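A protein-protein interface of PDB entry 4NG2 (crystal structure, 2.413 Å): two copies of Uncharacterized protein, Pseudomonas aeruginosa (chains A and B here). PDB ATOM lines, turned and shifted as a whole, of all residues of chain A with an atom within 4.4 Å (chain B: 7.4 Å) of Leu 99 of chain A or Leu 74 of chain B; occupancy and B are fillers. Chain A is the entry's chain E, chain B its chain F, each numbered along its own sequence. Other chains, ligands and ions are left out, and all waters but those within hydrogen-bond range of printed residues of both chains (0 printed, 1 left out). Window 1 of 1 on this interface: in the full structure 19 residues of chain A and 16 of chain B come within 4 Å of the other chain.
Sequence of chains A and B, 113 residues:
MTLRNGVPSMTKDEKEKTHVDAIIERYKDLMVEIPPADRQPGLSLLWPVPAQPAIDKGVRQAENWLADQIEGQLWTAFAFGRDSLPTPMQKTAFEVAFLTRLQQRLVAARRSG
NE2 of Gln 103 of chain A sits close to NE2 of Gln 73 of chain B (2.8 Å). OE1 of Gln 103 of chain A sits at hydrogen-bond distance from N of Leu 74 of chain B.
O of Val 96 of chain A sits at hydrogen-bond distance from OG1 of Thr 100 of chain A, at 2.9 Å. The indole nitrogen of Trp 65 of chain B is in hydrogen-bond range of the backbone carbonyl oxygen of Gly 72 of chain B (3.2 Å).
Among the printed residues, merely in contact across the chains: Gln 103 of chain A with Trp 65 of chain B, Leu 99 of chain A with Phe 78 of chain B, Leu 99 of chain A with Leu 74 of chain B, Phe 98 of chain A with Leu 99 of chain B, Leu 99 of chain A with Leu 102 of chain B, Val 96 of chain A with Trp 75 of chain B, Gln 103 of chain A with Ile 70 of chain B, Leu 102 of chain A with Leu 99 of chain B and Glu 95 of chain A with Phe 78 of chain B.
Of the printed residues of chain B, Glu 95 of chain A touches Phe 78 (3.98 Å). Of chain B, only Leu 74, Phe 78 and Leu 102 come within 4 Å of Leu 99 of chain A. Printed residues of chain B within 4 Å of Leu 102 of chain A: Leu 99 (3.9 Å). Of the printed residues of chain A, Trp 65 of chain B touches Gln 103. Of chain A, only Leu 99 and Gln 103 come within 4 Å of Leu 74 of chain B. Printed residues of chain A within 4 Å of Trp 75 of chain B: Val 96 (3.8 Å). The nearest printed residue of chain A that does not touch Leu 74 of chain B is Leu 102 of chain A (4.5 Å). The nearest printed residue of chain B that does not touch Glu 95 of chain A is Trp 75 of chain B (5.2 Å).
Of the 17 printed residues of chain B, 8 touch a printed residue of chain A. Hydrophobic or aromatic side chains of chain B that line the printed part of chain A: Trp 65, Ile 70, Leu 74, Trp 75, Phe 78, Leu 99 and Leu 102. Of the 9 printed residues of chain A, 6 touch a printed residue of chain B. Along chain A the printed residues that touch a printed residue of chain B span positions 95 to 103. Among the printed residues, no Asp or Glu carboxylate lies within 4 Å of a Lys or Arg side-chain nitrogen of the other chain.
Phe 98 of chain A touches Leu 99 of chain B, but with the chains exchanged Leu 99 of chain A does not touch Phe 98 of chain B (4.3 Å). Leu 99 of chain A touches Leu 102 of chain B, and with the chains exchanged Leu 102 of chain A touches Leu 99 of chain B.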
ATOM      1  N   GLU A  95      -3.789  27.393  23.268  1.00  0.00           N
ATOM      2  CA  GLU A  95      -2.572  27.611  24.048  1.00  0.00           C
ATOM      3  C   GLU A  95      -2.031  26.298  24.582  1.00  0.00           C
ATOM      4  O   GLU A  95      -0.825  26.047  24.539  1.00  0.00           O
ATOM      5  CB  GLU A  95      -2.836  28.528  25.238  1.00  0.00           C
ATOM      6  CG  GLU A  95      -3.362  29.894  24.884  1.00  0.00           C
ATOM      7  CD  GLU A  95      -3.673  30.731  26.112  1.00  0.00           C
ATOM      8  OE1 GLU A  95      -3.950  30.160  27.201  1.00  0.00           O
ATOM      9  OE2 GLU A  95      -3.635  31.967  25.987  1.00  0.00           O
ATOM     10  N   VAL A  96      -2.940  25.479  25.114  1.00  0.00           N
ATOM     11  CA  VAL A  96      -2.578  24.187  25.662  1.00  0.00           C
ATOM     12  C   VAL A  96      -1.948  23.319  24.560  1.00  0.00           C
ATOM     13  O   VAL A  96      -0.886  22.748  24.763  1.00  0.00           O
ATOM     14  CB  VAL A  96      -3.779  23.478  26.369  1.00  0.00           C
ATOM     15  CG1 VAL A  96      -3.434  22.039  26.719  1.00  0.00           C
ATOM     16  CG2 VAL A  96      -4.153  24.214  27.635  1.00  0.00           C
ATOM     17  N   ALA A  97      -2.565  23.267  23.383  1.00  0.00           N
ATOM     18  CA  ALA A  97      -2.037  22.434  22.296  1.00  0.00           C
ATOM     19  C   ALA A  97      -0.655  22.896  21.841  1.00  0.00           C
ATOM     20  O   ALA A  97       0.277  22.105  21.764  1.00  0.00           O
ATOM     21  CB  ALA A  97      -2.997  22.406  21.125  1.00  0.00           C
ATOM     22  N   PHE A  98      -0.539  24.191  21.560  1.00  0.00           N
ATOM     23  CA  PHE A  98       0.692  24.808  21.051  1.00  0.00           C
ATOM     24  C   PHE A  98       1.859  24.591  22.022  1.00  0.00           C
ATOM     25  O   PHE A  98       3.001  24.319  21.616  1.00  0.00           O
ATOM     26  CB  PHE A  98       0.405  26.297  20.835  1.00  0.00           C
ATOM     27  CG  PHE A  98       1.564  27.110  20.360  1.00  0.00           C
ATOM     28  CD1 PHE A  98       2.577  27.471  21.227  1.00  0.00           C
ATOM     29  CD2 PHE A  98       1.602  27.591  19.050  1.00  0.00           C
ATOM     30  CE1 PHE A  98       3.647  28.263  20.781  1.00  0.00           C
ATOM     31  CE2 PHE A  98       2.657  28.389  18.595  1.00  0.00           C
ATOM     32  CZ  PHE A  98       3.677  28.730  19.458  1.00  0.00           C
ATOM     33  N   LEU A  99       1.573  24.708  23.313  1.00  0.00           N
ATOM     34  CA  LEU A  99       2.617  24.570  24.321  1.00  0.00           C
ATOM     35  C   LEU A  99       2.991  23.104  24.527  1.00  0.00           C
ATOM     36  O   LEU A  99       4.154  22.783  24.690  1.00  0.00           O
ATOM     37  CB  LEU A  99       2.211  25.268  25.622  1.00  0.00           C
ATOM     38  CG  LEU A  99       2.448  26.786  25.533  1.00  0.00           C
ATOM     39  CD1 LEU A  99       1.549  27.598  26.460  1.00  0.00           C
ATOM     40  CD2 LEU A  99       3.904  27.107  25.807  1.00  0.00           C
ATOM     41  N   THR A 100       2.008  22.216  24.473  1.00  0.00           N
ATOM     42  CA  THR A 100       2.283  20.788  24.545  1.00  0.00           C
ATOM     43  C   THR A 100       3.187  20.346  23.399  1.00  0.00           C
ATOM     44  O   THR A 100       4.097  19.524  23.587  1.00  0.00           O
ATOM     45  CB  THR A 100       1.003  19.974  24.511  1.00  0.00           C
ATOM     46  OG1 THR A 100       0.268  20.221  25.710  1.00  0.00           O
ATOM     47  CG2 THR A 100       1.317  18.500  24.427  1.00  0.00           C
ATOM     48  N   ARG A 101       2.938  20.906  22.220  1.00  0.00           N
ATOM     49  CA  ARG A 101       3.789  20.664  21.063  1.00  0.00           C
ATOM     50  C   ARG A 101       5.204  21.206  21.271  1.00  0.00           C
ATOM     51  O   ARG A 101       6.168  20.587  20.824  1.00  0.00           O
ATOM     52  CB  ARG A 101       3.165  21.219  19.778  1.00  0.00           C
ATOM     53  CG  ARG A 101       3.880  20.734  18.527  1.00  0.00           C
ATOM     54  CD  ARG A 101       4.193  19.240  18.630  1.00  0.00           C
ATOM     55  NE  ARG A 101       5.022  18.746  17.531  1.00  0.00           N
ATOM     56  CZ  ARG A 101       6.348  18.600  17.582  1.00  0.00           C
ATOM     57  NH1 ARG A 101       7.023  18.910  18.680  1.00  0.00           N
ATOM     58  NH2 ARG A 101       7.006  18.142  16.524  1.00  0.00           N
ATOM     59  N   LEU A 102       5.342  22.345  21.949  1.00  0.00           N
ATOM     60  CA  LEU A 102       6.684  22.853  22.273  1.00  0.00           C
ATOM     61  C   LEU A 102       7.325  22.083  23.442  1.00  0.00           C
ATOM     62  O   LEU A 102       8.478  22.350  23.826  1.00  0.00           O
ATOM     63  CB  LEU A 102       6.667  24.340  22.624  1.00  0.00           C
ATOM     64  CG  LEU A 102       6.115  25.408  21.687  1.00  0.00           C
ATOM     65  CD1 LEU A 102       6.573  26.760  22.191  1.00  0.00           C
ATOM     66  CD2 LEU A 102       6.586  25.199  20.267  1.00  0.00           C
ATOM     67  N   GLN A 103       6.568  21.162  24.032  1.00  0.00           N
ATOM     68  CA  GLN A 103       7.080  20.336  25.116  1.00  0.00           C
ATOM     69  C   GLN A 103       7.588  19.041  24.497  1.00  0.00           C
ATOM     70  O   GLN A 103       8.755  18.672  24.659  1.00  0.00           O
ATOM     71  CB  GLN A 103       5.973  20.042  26.118  1.00  0.00           C
ATOM     72  CG  GLN A 103       6.181  18.789  26.959  1.00  0.00           C
ATOM     73  CD  GLN A 103       5.255  18.759  28.153  1.00  0.00           C
ATOM     74  OE1 GLN A 103       5.471  19.479  29.136  1.00  0.00           O
ATOM     75  NE2 GLN A 103       4.202  17.945  28.075  1.00  0.00           N
ATOM     76  N   GLN B  61       9.722  31.273  35.762  1.00  0.00           N
ATOM     77  CA  GLN B  61       8.762  30.190  35.613  1.00  0.00           C
ATOM     78  C   GLN B  61       9.175  29.208  34.503  1.00  0.00           C
ATOM     79  O   GLN B  61       9.080  27.993  34.668  1.00  0.00           O
ATOM     80  CB  GLN B  61       7.392  30.786  35.311  1.00  0.00           C
ATOM     81  CG  GLN B  61       6.251  29.813  35.413  1.00  0.00           C
ATOM     82  CD  GLN B  61       5.629  29.824  36.783  1.00  0.00           C
ATOM     83  OE1 GLN B  61       5.577  30.866  37.454  1.00  0.00           O
ATOM     84  NE2 GLN B  61       5.170  28.659  37.222  1.00  0.00           N
ATOM     85  N   ALA B  62       9.628  29.737  33.365  1.00  0.00           N
ATOM     86  CA  ALA B  62       9.989  28.880  32.233  1.00  0.00           C
ATOM     87  C   ALA B  62      11.280  28.100  32.515  1.00  0.00           C
ATOM     88  O   ALA B  62      11.337  26.868  32.333  1.00  0.00           O
ATOM     89  CB  ALA B  62      10.101  29.693  30.940  1.00  0.00           C
ATOM     90  N   TRP B  65      10.896  25.348  34.787  1.00  0.00           N
ATOM     91  CA  TRP B  65      10.374  24.164  34.111  1.00  0.00           C
ATOM     92  C   TRP B  65      11.449  23.463  33.305  1.00  0.00           C
ATOM     93  O   TRP B  65      11.502  22.240  33.276  1.00  0.00           O
ATOM     94  CB  TRP B  65       9.217  24.494  33.180  1.00  0.00           C
ATOM     95  CG  TRP B  65       8.657  23.254  32.578  1.00  0.00           C
ATOM     96  CD1 TRP B  65       7.667  22.481  33.088  1.00  0.00           C
ATOM     97  CD2 TRP B  65       9.069  22.629  31.357  1.00  0.00           C
ATOM     98  NE1 TRP B  65       7.423  21.407  32.256  1.00  0.00           N
ATOM     99  CE2 TRP B  65       8.276  21.474  31.188  1.00  0.00           C
ATOM    100  CE3 TRP B  65      10.026  22.942  30.381  1.00  0.00           C
ATOM    101  CZ2 TRP B  65       8.406  20.631  30.089  1.00  0.00           C
ATOM    102  CZ3 TRP B  65      10.158  22.101  29.294  1.00  0.00           C
ATOM    103  CH2 TRP B  65       9.356  20.957  29.157  1.00  0.00           C
ATOM    104  N   LEU B  66      12.283  24.231  32.612  1.00  0.00           N
ATOM    105  CA  LEU B  66      13.328  23.618  31.805  1.00  0.00           C
ATOM    106  C   LEU B  66      14.270  22.869  32.737  1.00  0.00           C
ATOM    107  O   LEU B  66      14.499  21.668  32.557  1.00  0.00           O
ATOM    108  CB  LEU B  66      14.075  24.645  30.951  1.00  0.00           C
ATOM    109  CG  LEU B  66      13.341  25.281  29.759  1.00  0.00           C
ATOM    110  CD1 LEU B  66      14.171  26.404  29.154  1.00  0.00           C
ATOM    111  CD2 LEU B  66      12.950  24.261  28.674  1.00  0.00           C
ATOM    112  N   ILE B  70      10.787  17.557  33.210  1.00  0.00           N
ATOM    113  CA  ILE B  70       9.355  17.243  33.157  1.00  0.00           C
ATOM    114  C   ILE B  70       8.843  16.398  34.340  1.00  0.00           C
ATOM    115  O   ILE B  70       9.057  15.185  34.403  1.00  0.00           O
ATOM    116  CB  ILE B  70       8.955  16.611  31.779  1.00  0.00           C
ATOM    117  CG1 ILE B  70       7.434  16.603  31.589  1.00  0.00           C
ATOM    118  CG2 ILE B  70       9.561  15.216  31.610  1.00  0.00           C
ATOM    119  CD1 ILE B  70       6.991  15.979  30.279  1.00  0.00           C
ATOM    120  N   GLY B  72       5.800  17.999  35.684  1.00  0.00           N
ATOM    121  CA  GLY B  72       4.466  18.487  35.388  1.00  0.00           C
ATOM    122  C   GLY B  72       4.437  18.972  33.954  1.00  0.00           C
ATOM    123  O   GLY B  72       5.493  19.157  33.354  1.00  0.00           O
ATOM    124  N   GLN B  73       3.239  19.163  33.401  1.00  0.00           N
ATOM    125  CA  GLN B  73       3.082  19.672  32.031  1.00  0.00           C
ATOM    126  C   GLN B  73       3.592  21.110  31.886  1.00  0.00           C
ATOM    127  O   GLN B  73       3.490  21.915  32.821  1.00  0.00           O
ATOM    128  CB  GLN B  73       1.614  19.620  31.593  1.00  0.00           C
ATOM    129  CG  GLN B  73       1.054  18.231  31.351  1.00  0.00           C
ATOM    130  CD  GLN B  73       1.826  17.483  30.279  1.00  0.00           C
ATOM    131  OE1 GLN B  73       2.638  16.598  30.587  1.00  0.00           O
ATOM    132  NE2 GLN B  73       1.579  17.830  29.008  1.00  0.00           N
ATOM    133  N   LEU B  74       4.134  21.428  30.709  1.00  0.00           N
ATOM    134  CA  LEU B  74       4.609  22.778  30.425  1.00  0.00           C
ATOM    135  C   LEU B  74       3.419  23.723  30.302  1.00  0.00           C
ATOM    136  O   LEU B  74       3.487  24.910  30.656  1.00  0.00           O
ATOM    137  CB  LEU B  74       5.411  22.798  29.137  1.00  0.00           C
ATOM    138  CG  LEU B  74       5.922  24.180  28.768  1.00  0.00           C
ATOM    139  CD1 LEU B  74       7.125  24.477  29.609  1.00  0.00           C
ATOM    140  CD2 LEU B  74       6.278  24.225  27.306  1.00  0.00           C
ATOM    141  N   TRP B  75       2.318  23.196  29.799  1.00  0.00           N
ATOM    142  CA  TRP B  75       1.134  24.022  29.659  1.00  0.00           C
ATOM    143  C   TRP B  75       0.711  24.502  31.042  1.00  0.00           C
ATOM    144  O   TRP B  75       0.408  25.688  31.243  1.00  0.00           O
ATOM    145  CB  TRP B  75       0.021  23.291  28.889  1.00  0.00           C
ATOM    146  CG  TRP B  75      -0.845  22.358  29.669  1.00  0.00           C
ATOM    147  CD1 TRP B  75      -0.833  20.996  29.618  1.00  0.00           C
ATOM    148  CD2 TRP B  75      -1.888  22.717  30.575  1.00  0.00           C
ATOM    149  NE1 TRP B  75      -1.803  20.483  30.438  1.00  0.00           N
ATOM    150  CE2 TRP B  75      -2.463  21.521  31.044  1.00  0.00           C
ATOM    151  CE3 TRP B  75      -2.397  23.935  31.034  1.00  0.00           C
ATOM    152  CZ2 TRP B  75      -3.512  21.508  31.968  1.00  0.00           C
ATOM    153  CZ3 TRP B  75      -3.442  23.922  31.938  1.00  0.00           C
ATOM    154  CH2 TRP B  75      -3.984  22.715  32.403  1.00  0.00           C
ATOM    155  N   THR B  76       0.749  23.581  32.000  1.00  0.00           N
ATOM    156  CA  THR B  76       0.452  23.885  33.385  1.00  0.00           C
ATOM    157  C   THR B  76       1.308  24.997  33.968  1.00  0.00           C
ATOM    158  O   THR B  76       0.809  25.827  34.717  1.00  0.00           O
ATOM    159  CB  THR B  76       0.633  22.656  34.240  1.00  0.00           C
ATOM    160  OG1 THR B  76      -0.111  21.592  33.653  1.00  0.00           O
ATOM    161  CG2 THR B  76       0.128  22.909  35.644  1.00  0.00           C
ATOM    162  N   ALA B  77       2.593  25.027  33.650  1.00  0.00           N
ATOM    163  CA  ALA B  77       3.442  26.050  34.254  1.00  0.00           C
ATOM    164  C   ALA B  77       3.113  27.407  33.658  1.00  0.00           C
ATOM    165  O   ALA B  77       3.266  28.430  34.314  1.00  0.00           O
ATOM    166  CB  ALA B  77       4.909  25.723  34.056  1.00  0.00           C
ATOM    167  N   PHE B  78       2.672  27.395  32.402  1.00  0.00           N
ATOM    168  CA  PHE B  78       2.287  28.600  31.674  1.00  0.00           C
ATOM    169  C   PHE B  78       0.967  29.155  32.203  1.00  0.00           C
ATOM    170  O   PHE B  78       0.901  30.316  32.607  1.00  0.00           O
ATOM    171  CB  PHE B  78       2.178  28.281  30.171  1.00  0.00           C
ATOM    172  CG  PHE B  78       1.671  29.423  29.326  1.00  0.00           C
ATOM    173  CD1 PHE B  78       2.552  30.322  28.759  1.00  0.00           C
ATOM    174  CD2 PHE B  78       0.316  29.576  29.085  1.00  0.00           C
ATOM    175  CE1 PHE B  78       2.097  31.357  27.988  1.00  0.00           C
ATOM    176  CE2 PHE B  78      -0.153  30.612  28.307  1.00  0.00           C
ATOM    177  CZ  PHE B  78       0.735  31.505  27.757  1.00  0.00           C
ATOM    178  N   ALA B  79      -0.067  28.313  32.223  1.00  0.00           N
ATOM    179  CA  ALA B  79      -1.411  28.722  32.632  1.00  0.00           C
ATOM    180  C   ALA B  79      -1.504  29.067  34.110  1.00  0.00           C
ATOM    181  O   ALA B  79      -1.993  30.133  34.470  1.00  0.00           O
ATOM    182  CB  ALA B  79      -2.439  27.651  32.280  1.00  0.00           C
ATOM    183  N   PHE B  80      -1.054  28.178  34.980  1.00  0.00           N
ATOM    184  CA  PHE B  80      -1.105  28.500  36.403  1.00  0.00           C
ATOM    185  C   PHE B  80      -0.179  29.674  36.727  1.00  0.00           C
ATOM    186  O   PHE B  80      -0.447  30.432  37.632  1.00  0.00           O
ATOM    187  CB  PHE B  80      -0.798  27.272  37.273  1.00  0.00           C
ATOM    188  CG  PHE B  80      -1.948  26.301  37.398  1.00  0.00           C
ATOM    189  CD1 PHE B  80      -2.172  25.351  36.443  1.00  0.00           C
ATOM    190  CD2 PHE B  80      -2.788  26.340  38.489  1.00  0.00           C
ATOM    191  CE1 PHE B  80      -3.218  24.449  36.563  1.00  0.00           C
ATOM    192  CE2 PHE B  80      -3.838  25.453  38.614  1.00  0.00           C
ATOM    193  CZ  PHE B  80      -4.055  24.503  37.648  1.00  0.00           C
ATOM    194  N   PHE B  98       7.819  34.101  29.099  1.00  0.00           N
ATOM    195  CA  PHE B  98       7.758  32.639  29.103  1.00  0.00           C
ATOM    196  C   PHE B  98       8.034  32.038  27.726  1.00  0.00           C
ATOM    197  O   PHE B  98       8.858  31.126  27.594  1.00  0.00           O
ATOM    198  CB  PHE B  98       6.387  32.204  29.572  1.00  0.00           C
ATOM    199  CG  PHE B  98       6.292  30.764  29.975  1.00  0.00           C
ATOM    200  CD1 PHE B  98       6.465  30.395  31.292  1.00  0.00           C
ATOM    201  CD2 PHE B  98       5.947  29.794  29.049  1.00  0.00           C
ATOM    202  CE1 PHE B  98       6.322  29.082  31.681  1.00  0.00           C
ATOM    203  CE2 PHE B  98       5.791  28.479  29.419  1.00  0.00           C
ATOM    204  CZ  PHE B  98       5.983  28.117  30.739  1.00  0.00           C
ATOM    205  N   LEU B  99       7.346  32.531  26.695  1.00  0.00           N
ATOM    206  CA  LEU B  99       7.543  31.987  25.353  1.00  0.00           C
ATOM    207  C   LEU B  99       8.914  32.337  24.761  1.00  0.00           C
ATOM    208  O   LEU B  99       9.539  31.495  24.120  1.00  0.00           O
ATOM    209  CB  LEU B  99       6.408  32.374  24.414  1.00  0.00           C
ATOM    210  CG  LEU B  99       5.222  31.403  24.455  1.00  0.00           C
ATOM    211  CD1 LEU B  99       3.924  32.144  24.269  1.00  0.00           C
ATOM    212  CD2 LEU B  99       5.347  30.312  23.402  1.00  0.00           C
ATOM    213  N   LEU B 102      11.399  29.877  26.265  1.00  0.00           N
ATOM    214  CA  LEU B 102      11.303  28.617  25.545  1.00  0.00           C
ATOM    215  C   LEU B 102      11.998  28.742  24.190  1.00  0.00           C
ATOM    216  O   LEU B 102      12.778  27.867  23.803  1.00  0.00           O
ATOM    217  CB  LEU B 102       9.850  28.204  25.333  1.00  0.00           C
ATOM    218  CG  LEU B 102       9.020  27.838  26.553  1.00  0.00           C
ATOM    219  CD1 LEU B 102       7.679  27.287  26.084  1.00  0.00           C
ATOM    220  CD2 LEU B 102       9.755  26.819  27.376  1.00  0.00           C
